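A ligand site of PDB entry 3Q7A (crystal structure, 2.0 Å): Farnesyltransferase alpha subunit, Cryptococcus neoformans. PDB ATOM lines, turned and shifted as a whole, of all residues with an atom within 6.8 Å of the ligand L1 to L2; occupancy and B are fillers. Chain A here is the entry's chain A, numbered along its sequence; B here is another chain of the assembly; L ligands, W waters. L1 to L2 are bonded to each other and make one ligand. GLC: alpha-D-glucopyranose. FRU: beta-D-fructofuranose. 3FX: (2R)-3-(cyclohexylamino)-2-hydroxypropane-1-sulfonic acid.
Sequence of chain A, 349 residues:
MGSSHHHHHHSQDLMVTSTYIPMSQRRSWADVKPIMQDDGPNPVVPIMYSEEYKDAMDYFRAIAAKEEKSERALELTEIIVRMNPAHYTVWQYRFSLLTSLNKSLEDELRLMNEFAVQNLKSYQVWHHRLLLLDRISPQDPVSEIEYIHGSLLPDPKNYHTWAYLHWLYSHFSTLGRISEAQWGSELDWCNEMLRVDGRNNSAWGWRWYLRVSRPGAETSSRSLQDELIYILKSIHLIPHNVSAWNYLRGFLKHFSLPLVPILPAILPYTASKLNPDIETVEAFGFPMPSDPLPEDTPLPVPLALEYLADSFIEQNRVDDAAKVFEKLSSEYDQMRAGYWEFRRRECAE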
ATOM      1  N   PHE A  60      -8.217 -10.171  -9.985  1.00  0.00           N
ATOM      2  CA  PHE A  60      -7.103 -10.976 -10.499  1.00  0.00           C
ATOM      3  C   PHE A  60      -6.757 -12.115  -9.556  1.00  0.00           C
ATOM      4  O   PHE A  60      -6.522 -13.248 -10.006  1.00  0.00           O
ATOM      5  CB  PHE A  60      -5.859 -10.129 -10.784  1.00  0.00           C
ATOM      6  CG  PHE A  60      -4.661 -10.951 -11.200  1.00  0.00           C
ATOM      7  CD1 PHE A  60      -4.544 -11.435 -12.507  1.00  0.00           C
ATOM      8  CD2 PHE A  60      -3.661 -11.258 -10.284  1.00  0.00           C
ATOM      9  CE1 PHE A  60      -3.457 -12.204 -12.892  1.00  0.00           C
ATOM     10  CE2 PHE A  60      -2.560 -12.028 -10.659  1.00  0.00           C
ATOM     11  CZ  PHE A  60      -2.457 -12.508 -11.967  1.00  0.00           C
ATOM     12  N   ALA A  64      -6.770 -15.802 -10.937  1.00  0.00           N
ATOM     13  CA  ALA A  64      -5.545 -16.587 -10.948  1.00  0.00           C
ATOM     14  C   ALA A  64      -5.620 -17.820 -10.041  1.00  0.00           C
ATOM     15  O   ALA A  64      -5.083 -18.880 -10.394  1.00  0.00           O
ATOM     16  CB  ALA A  64      -4.340 -15.721 -10.576  1.00  0.00           C
ATOM     17  N   ALA A  65      -6.278 -17.684  -8.896  1.00  0.00           N
ATOM     18  CA  ALA A  65      -6.480 -18.809  -7.980  1.00  0.00           C
ATOM     19  C   ALA A  65      -7.273 -19.946  -8.620  1.00  0.00           C
ATOM     20  O   ALA A  65      -6.943 -21.113  -8.445  1.00  0.00           O
ATOM     21  CB  ALA A  65      -7.155 -18.335  -6.691  1.00  0.00           C
ATOM     22  N   GLU A  67      -7.460 -20.282 -11.818  1.00  0.00           N
ATOM     23  CA  GLU A  67      -6.748 -20.518 -13.079  1.00  0.00           C
ATOM     24  C   GLU A  67      -7.625 -20.396 -14.330  1.00  0.00           C
ATOM     25  O   GLU A  67      -7.522 -21.192 -15.268  1.00  0.00           O
ATOM     26  CB  GLU A  67      -5.975 -21.851 -13.055  1.00  0.00           C
ATOM     27  CG  GLU A  67      -4.899 -21.906 -11.967  1.00  0.00           C
ATOM     28  CD  GLU A  67      -3.956 -23.088 -12.094  1.00  0.00           C
ATOM     29  OE1 GLU A  67      -4.403 -24.187 -12.505  1.00  0.00           O
ATOM     30  OE2 GLU A  67      -2.752 -22.921 -11.781  1.00  0.00           O
ATOM     31  N   LYS A  69      -8.746 -19.181 -17.793  1.00  0.00           N
ATOM     32  CA  LYS A  69      -8.141 -18.713 -19.033  1.00  0.00           C
ATOM     33  C   LYS A  69      -9.247 -18.254 -19.971  1.00  0.00           C
ATOM     34  O   LYS A  69      -9.857 -19.050 -20.679  1.00  0.00           O
ATOM     35  CB  LYS A  69      -7.294 -19.818 -19.673  1.00  0.00           C
ATOM     36  CG  LYS A  69      -6.201 -20.378 -18.768  1.00  0.00           C
ATOM     37  CD  LYS A  69      -5.001 -19.447 -18.683  1.00  0.00           C
ATOM     38  CE  LYS A  69      -4.411 -19.415 -17.289  1.00  0.00           C
ATOM     39  NZ  LYS A  69      -4.164 -20.764 -16.685  1.00  0.00           N
ATOM     40  N   THR A  89       4.026 -11.082 -11.948  1.00  0.00           N
ATOM     41  CA  THR A  89       3.018 -12.128 -11.773  1.00  0.00           C
ATOM     42  C   THR A  89       1.932 -12.036 -12.843  1.00  0.00           C
ATOM     43  O   THR A  89       1.524 -13.035 -13.440  1.00  0.00           O
ATOM     44  CB  THR A  89       2.388 -12.078 -10.366  1.00  0.00           C
ATOM     45  OG1 THR A  89       3.407 -12.242  -9.369  1.00  0.00           O
ATOM     46  CG2 THR A  89       1.315 -13.173 -10.176  1.00  0.00           C
ATOM     47  N   GLN A  92       3.291 -12.884 -16.343  1.00  0.00           N
ATOM     48  CA  GLN A  92       3.361 -14.348 -16.448  1.00  0.00           C
ATOM     49  C   GLN A  92       1.992 -14.908 -16.792  1.00  0.00           C
ATOM     50  O   GLN A  92       1.863 -15.773 -17.661  1.00  0.00           O
ATOM     51  CB  GLN A  92       3.877 -14.952 -15.131  1.00  0.00           C
ATOM     52  CG  GLN A  92       4.293 -16.423 -15.218  1.00  0.00           C
ATOM     53  CD  GLN A  92       3.124 -17.397 -15.146  1.00  0.00           C
ATOM     54  OE1 GLN A  92       2.097 -17.126 -14.515  1.00  0.00           O
ATOM     55  NE2 GLN A  92       3.281 -18.556 -15.785  1.00  0.00           N
ATOM     56  N   TYR A  93       0.953 -14.400 -16.107  1.00  0.00           N
ATOM     57  CA  TYR A  93      -0.406 -14.835 -16.351  1.00  0.00           C
ATOM     58  C   TYR A  93      -0.897 -14.436 -17.747  1.00  0.00           C
ATOM     59  O   TYR A  93      -1.595 -15.198 -18.408  1.00  0.00           O
ATOM     60  CB  TYR A  93      -1.367 -14.318 -15.275  1.00  0.00           C
ATOM     61  CG  TYR A  93      -2.592 -15.204 -15.116  1.00  0.00           C
ATOM     62  CD1 TYR A  93      -2.567 -16.308 -14.270  1.00  0.00           C
ATOM     63  CD2 TYR A  93      -3.769 -14.934 -15.818  1.00  0.00           C
ATOM     64  CE1 TYR A  93      -3.673 -17.145 -14.130  1.00  0.00           C
ATOM     65  CE2 TYR A  93      -4.888 -15.766 -15.679  1.00  0.00           C
ATOM     66  CZ  TYR A  93      -4.835 -16.856 -14.831  1.00  0.00           C
ATOM     67  OH  TYR A  93      -5.922 -17.682 -14.686  1.00  0.00           O
ATOM     68  N   ARG A  94      -0.505 -13.230 -18.190  1.00  0.00           N
ATOM     69  CA  ARG A  94      -0.881 -12.739 -19.514  1.00  0.00           C
ATOM     70  C   ARG A  94      -0.356 -13.640 -20.637  1.00  0.00           C
ATOM     71  O   ARG A  94      -1.079 -13.955 -21.567  1.00  0.00           O
ATOM     72  CB  ARG A  94      -0.438 -11.293 -19.724  1.00  0.00           C
ATOM     73  CG  ARG A  94      -0.802 -10.764 -21.119  1.00  0.00           C
ATOM     74  CD  ARG A  94      -0.639  -9.262 -21.265  1.00  0.00           C
ATOM     75  NE  ARG A  94      -1.183  -8.820 -22.544  1.00  0.00           N
ATOM     76  CZ  ARG A  94      -2.442  -8.462 -22.756  1.00  0.00           C
ATOM     77  NH1 ARG A  94      -3.319  -8.469 -21.751  1.00  0.00           N
ATOM     78  NH2 ARG A  94      -2.831  -8.095 -23.962  1.00  0.00           N
ATOM     79  N   PHE A  95       0.916 -14.046 -20.536  1.00  0.00           N
ATOM     80  CA  PHE A  95       1.489 -14.920 -21.554  1.00  0.00           C
ATOM     81  C   PHE A  95       0.816 -16.285 -21.588  1.00  0.00           C
ATOM     82  O   PHE A  95       0.597 -16.840 -22.665  1.00  0.00           O
ATOM     83  CB  PHE A  95       3.009 -15.051 -21.402  1.00  0.00           C
ATOM     84  CG  PHE A  95       3.681 -15.691 -22.601  1.00  0.00           C
ATOM     85  CD1 PHE A  95       3.975 -14.940 -23.727  1.00  0.00           C
ATOM     86  CD2 PHE A  95       4.002 -17.050 -22.585  1.00  0.00           C
ATOM     87  CE1 PHE A  95       4.582 -15.531 -24.843  1.00  0.00           C
ATOM     88  CE2 PHE A  95       4.605 -17.650 -23.686  1.00  0.00           C
ATOM     89  CZ  PHE A  95       4.904 -16.887 -24.817  1.00  0.00           C
ATOM     90  N   SER A  96       0.483 -16.813 -20.410  1.00  0.00           N
ATOM     91  CA  SER A  96      -0.287 -18.060 -20.289  1.00  0.00           C
ATOM     92  C   SER A  96      -1.644 -17.940 -20.981  1.00  0.00           C
ATOM     93  O   SER A  96      -2.114 -18.888 -21.615  1.00  0.00           O
ATOM     94  CB  SER A  96      -0.498 -18.449 -18.831  1.00  0.00           C
ATOM     95  OG  SER A  96       0.731 -18.799 -18.219  1.00  0.00           O
ATOM     96  N   LEU A  97      -2.263 -16.763 -20.833  1.00  0.00           N
ATOM     97  CA  LEU A  97      -3.543 -16.474 -21.482  1.00  0.00           C
ATOM     98  C   LEU A  97      -3.419 -16.417 -23.001  1.00  0.00           C
ATOM     99  O   LEU A  97      -4.285 -16.919 -23.724  1.00  0.00           O
ATOM    100  CB  LEU A  97      -4.130 -15.169 -20.944  1.00  0.00           C
ATOM    101  CG  LEU A  97      -4.762 -15.205 -19.545  1.00  0.00           C
ATOM    102  CD1 LEU A  97      -4.900 -13.803 -18.997  1.00  0.00           C
ATOM    103  CD2 LEU A  97      -6.117 -15.900 -19.585  1.00  0.00           C
ATOM    104  N   SER A 100      -2.963 -20.104 -24.159  1.00  0.00           N
ATOM    105  CA  SER A 100      -4.186 -20.886 -23.913  1.00  0.00           C
ATOM    106  C   SER A 100      -5.311 -20.540 -24.880  1.00  0.00           C
ATOM    107  O   SER A 100      -5.985 -21.422 -25.395  1.00  0.00           O
ATOM    108  CB  SER A 100      -4.696 -20.699 -22.475  1.00  0.00           C
ATOM    109  OG  SER A 100      -3.732 -21.131 -21.537  1.00  0.00           O
ATOM    110  N   SER B 123       5.631 -18.227  -0.189  1.00  0.00           N
ATOM    111  CA  SER B 123       4.772 -19.292  -0.712  1.00  0.00           C
ATOM    112  C   SER B 123       5.204 -20.649  -0.174  1.00  0.00           C
ATOM    113  O   SER B 123       6.400 -20.925  -0.099  1.00  0.00           O
ATOM    114  CB  SER B 123       4.796 -19.321  -2.242  1.00  0.00           C
ATOM    115  OG  SER B 123       4.187 -18.168  -2.791  1.00  0.00           O
ATOM    116  N   LYS B 125       5.091 -23.371  -1.686  1.00  0.00           N
ATOM    117  CA  LYS B 125       5.811 -24.038  -2.769  1.00  0.00           C
ATOM    118  C   LYS B 125       7.288 -23.640  -2.832  1.00  0.00           C
ATOM    119  O   LYS B 125       8.091 -24.312  -3.475  1.00  0.00           O
ATOM    120  CB  LYS B 125       5.147 -23.761  -4.122  1.00  0.00           C
ATOM    121  CG  LYS B 125       3.750 -24.336  -4.285  1.00  0.00           C
ATOM    122  CD  LYS B 125       3.738 -25.799  -4.687  1.00  0.00           C
ATOM    123  CE  LYS B 125       2.325 -26.266  -4.980  1.00  0.00           C
ATOM    124  NZ  LYS B 125       2.289 -27.634  -5.562  1.00  0.00           N
ATOM    125  N   ALA B 133       1.624 -14.084  -0.785  1.00  0.00           N
ATOM    126  CA  ALA B 133       1.605 -15.333  -1.569  1.00  0.00           C
ATOM    127  C   ALA B 133       0.309 -15.530  -2.373  1.00  0.00           C
ATOM    128  O   ALA B 133       0.316 -16.218  -3.402  1.00  0.00           O
ATOM    129  CB  ALA B 133       1.847 -16.533  -0.657  1.00  0.00           C
ATOM    130  N   SER B 135      -1.155 -13.166  -3.908  1.00  0.00           N
ATOM    131  CA  SER B 135      -1.169 -12.028  -4.834  1.00  0.00           C
ATOM    132  C   SER B 135      -0.059 -12.078  -5.877  1.00  0.00           C
ATOM    133  O   SER B 135      -0.255 -11.630  -7.013  1.00  0.00           O
ATOM    134  CB  SER B 135      -1.078 -10.711  -4.051  1.00  0.00           C
ATOM    135  OG  SER B 135      -2.124 -10.598  -3.104  1.00  0.00           O
ATOM    136  N   GLN B 136       1.106 -12.598  -5.482  1.00  0.00           N
ATOM    137  CA  GLN B 136       2.279 -12.624  -6.356  1.00  0.00           C
ATOM    138  C   GLN B 136       3.024 -13.956  -6.264  1.00  0.00           C
ATOM    139  O   GLN B 136       3.078 -14.568  -5.202  1.00  0.00           O
ATOM    140  CB  GLN B 136       3.226 -11.454  -6.035  1.00  0.00           C
ATOM    141  CG  GLN B 136       2.601 -10.071  -6.233  1.00  0.00           C
ATOM    142  CD  GLN B 136       3.592  -8.918  -6.072  1.00  0.00           C
ATOM    143  OE1 GLN B 136       3.294  -7.907  -5.435  1.00  0.00           O
ATOM    144  NE2 GLN B 136       4.769  -9.070  -6.665  1.00  0.00           N
ATOM    145  N   ILE B 137       3.603 -14.386  -7.380  1.00  0.00           N
ATOM    146  CA  ILE B 137       4.378 -15.631  -7.436  1.00  0.00           C
ATOM    147  C   ILE B 137       5.812 -15.400  -6.928  1.00  0.00           C
ATOM    148  O   ILE B 137       6.275 -14.261  -6.893  1.00  0.00           O
ATOM    149  CB  ILE B 137       4.384 -16.272  -8.864  1.00  0.00           C
ATOM    150  CG1 ILE B 137       4.979 -15.316  -9.914  1.00  0.00           C
ATOM    151  CG2 ILE B 137       2.967 -16.708  -9.256  1.00  0.00           C
ATOM    152  CD1 ILE B 137       5.204 -15.930 -11.294  1.00  0.00           C
ATOM    153  N   PRO B 138       6.497 -16.478  -6.492  1.00  0.00           N
ATOM    154  CA  PRO B 138       7.875 -16.333  -5.988  1.00  0.00           C
ATOM    155  C   PRO B 138       8.841 -15.819  -7.058  1.00  0.00           C
ATOM    156  O   PRO B 138       8.642 -16.036  -8.255  1.00  0.00           O
ATOM    157  CB  PRO B 138       8.250 -17.764  -5.578  1.00  0.00           C
ATOM    158  CG  PRO B 138       6.953 -18.446  -5.346  1.00  0.00           C
ATOM    159  CD  PRO B 138       5.999 -17.858  -6.317  1.00  0.00           C
ATOM    160  N   GLU B 190       9.009 -17.951 -12.613  1.00  0.00           N
ATOM    161  CA  GLU B 190       8.392 -18.759 -13.651  1.00  0.00           C
ATOM    162  C   GLU B 190       8.106 -17.896 -14.876  1.00  0.00           C
ATOM    163  O   GLU B 190       7.442 -16.861 -14.774  1.00  0.00           O
ATOM    164  CB  GLU B 190       7.111 -19.416 -13.127  1.00  0.00           C
ATOM    165  CG  GLU B 190       6.552 -20.477 -14.044  1.00  0.00           C
ATOM    166  CD  GLU B 190       5.570 -21.403 -13.334  1.00  0.00           C
ATOM    167  OE1 GLU B 190       5.083 -21.054 -12.236  1.00  0.00           O
ATOM    168  OE2 GLU B 190       5.288 -22.482 -13.896  1.00  0.00           O
HETATM  169  C1  GLC L   1       1.482 -20.433 -12.068  1.00  0.00           C
HETATM  170  C2  GLC L   1       2.146 -20.709 -10.715  1.00  0.00           C
HETATM  171  C3  GLC L   1       1.101 -20.871  -9.600  1.00  0.00           C
HETATM  172  C4  GLC L   1       0.126 -19.692  -9.567  1.00  0.00           C
HETATM  173  C5  GLC L   1      -0.442 -19.377 -10.965  1.00  0.00           C
HETATM  174  C6  GLC L   1      -1.238 -18.059 -10.970  1.00  0.00           C
HETATM  175  O2  GLC L   1       2.956 -21.891 -10.800  1.00  0.00           O
HETATM  176  O3  GLC L   1       1.750 -20.988  -8.333  1.00  0.00           O
HETATM  177  O4  GLC L   1      -0.948 -19.993  -8.663  1.00  0.00           O
HETATM  178  O5  GLC L   1       0.603 -19.275 -11.990  1.00  0.00           O
HETATM  179  O6  GLC L   1      -0.370 -16.961 -10.679  1.00  0.00           O
HETATM  180  C1  FRU L   2       2.219 -22.831 -14.053  1.00  0.00           C
HETATM  181  C2  FRU L   2       0.931 -22.021 -13.896  1.00  0.00           C
HETATM  182  C3  FRU L   2      -0.270 -22.853 -14.337  1.00  0.00           C
HETATM  183  C4  FRU L   2      -1.292 -21.762 -14.599  1.00  0.00           C
HETATM  184  C5  FRU L   2      -0.430 -20.744 -15.348  1.00  0.00           C
HETATM  185  C6  FRU L   2      -0.950 -19.339 -15.064  1.00  0.00           C
HETATM  186  O1  FRU L   2       2.633 -22.841 -15.427  1.00  0.00           O
HETATM  187  O2  FRU L   2       0.754 -21.616 -12.509  1.00  0.00           O
HETATM  188  O3  FRU L   2      -0.707 -23.686 -13.252  1.00  0.00           O
HETATM  189  O4  FRU L   2      -2.322 -22.261 -15.451  1.00  0.00           O
HETATM  190  O5  FRU L   2       0.923 -20.884 -14.800  1.00  0.00           O
HETATM  191  O6  FRU L   2      -0.055 -18.370 -15.611  1.00  0.00           O
HETATM  192  OAA 3FX L   3       2.125 -21.627  -4.182  1.00  0.00           O
HETATM  193  OAB 3FX L   3       0.583 -23.530  -3.978  1.00  0.00           O
HETATM  194  OAC 3FX L   3      -0.184 -21.362  -5.661  1.00  0.00           O
HETATM  195  OAD 3FX L   3       1.558 -22.530  -2.038  1.00  0.00           O
HETATM  196  CAE 3FX L   3      -1.707 -14.908  -7.940  1.00  0.00           C
HETATM  197  CAF 3FX L   3      -2.888 -15.530  -7.167  1.00  0.00           C
HETATM  198  CAG 3FX L   3      -0.362 -15.243  -7.278  1.00  0.00           C
HETATM  199  CAH 3FX L   3      -2.693 -17.033  -6.940  1.00  0.00           C
HETATM  200  CAI 3FX L   3      -0.189 -16.741  -7.041  1.00  0.00           C
HETATM  201  CAJ 3FX L   3      -0.698 -19.157  -4.808  1.00  0.00           C
HETATM  202  CAK 3FX L   3      -0.357 -21.077  -3.237  1.00  0.00           C
HETATM  203  NAL 3FX L   3      -1.196 -18.784  -6.138  1.00  0.00           N
HETATM  204  CAM 3FX L   3      -0.881 -20.664  -4.615  1.00  0.00           C
HETATM  205  CAN 3FX L   3      -1.362 -17.335  -6.236  1.00  0.00           C
HETATM  206  SAO 3FX L   3       1.046 -22.246  -3.342  1.00  0.00           S
HETATM  207  O   HOH W   1       5.158 -23.808  -9.551  1.00  0.00           O
HETATM  208  O   HOH W   2       1.619 -24.185 -10.961  1.00  0.00           O
HETATM  209  O   HOH W   3       5.493 -19.731  -9.853  1.00  0.00           O
HETATM  210  O   HOH W   4       3.077 -23.348  -7.885  1.00  0.00           O
HETATM  211  O   HOH W   5       0.914 -15.631 -12.578  1.00  0.00           O
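O3 of FRU L2 lies within hydrogen-bond range of OE2 of Glu 67. The side-chain amino group (NZ) of Lys 69 is in hydrogen-bond range of an oxygen (O4) of FRU L2. The side-chain carboxylate (OE1) of Glu 190 of chain B is in hydrogen-bond range of an oxygen (O2) of GLC L1 (2.7 Å). O6 of FRU L2 is in hydrogen-bond range of OE1 of Gln 92 (2.7 Å). OG of Ser 96 lies within hydrogen-bond range of O6 of FRU L2 (2.8 Å).
NAL of 3FX L3 sits at hydrogen-bond distance from O4 of GLC L1 (2.8 Å).
O of Gln 92 lies within hydrogen-bond range of OG of Ser 96 (3.3 Å). OG of Ser 100 sits at hydrogen-bond distance from O of Ser 96. N of Ile 137 of chain B is in hydrogen-bond range of OG1 of Thr 89 (2.9 Å).
CB of Ala 64 touches C6 of GLC L1, at 3.9 Å. CD1 of Tyr 93 touches O6 of FRU L2 (3.5 Å). CG2 of Ile 137 of chain B touches O6 of GLC L1, at 3.6 Å. Hydrophobic or aromatic side chains that line the ligand L1 to L2: Ala 64, Tyr 93 and Ile 137 of chain B. Of the 21 residues printed, 8 come within 4 Å of the ligand L1 to L2. The nearest printed residue that does not touch the ligand L1 to L2 is Thr 89 (4.2 Å).
Water W5 lies within hydrogen-bond range of O6 of GLC L1 (2.7 Å), OE1 of Gln 92 (2.7 Å) and O of Thr 89 (2.8 Å). Water W3 bridges OE1 of Glu 190 of chain B (2.8 Å) and O2 of GLC L1 (3.5 Å).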
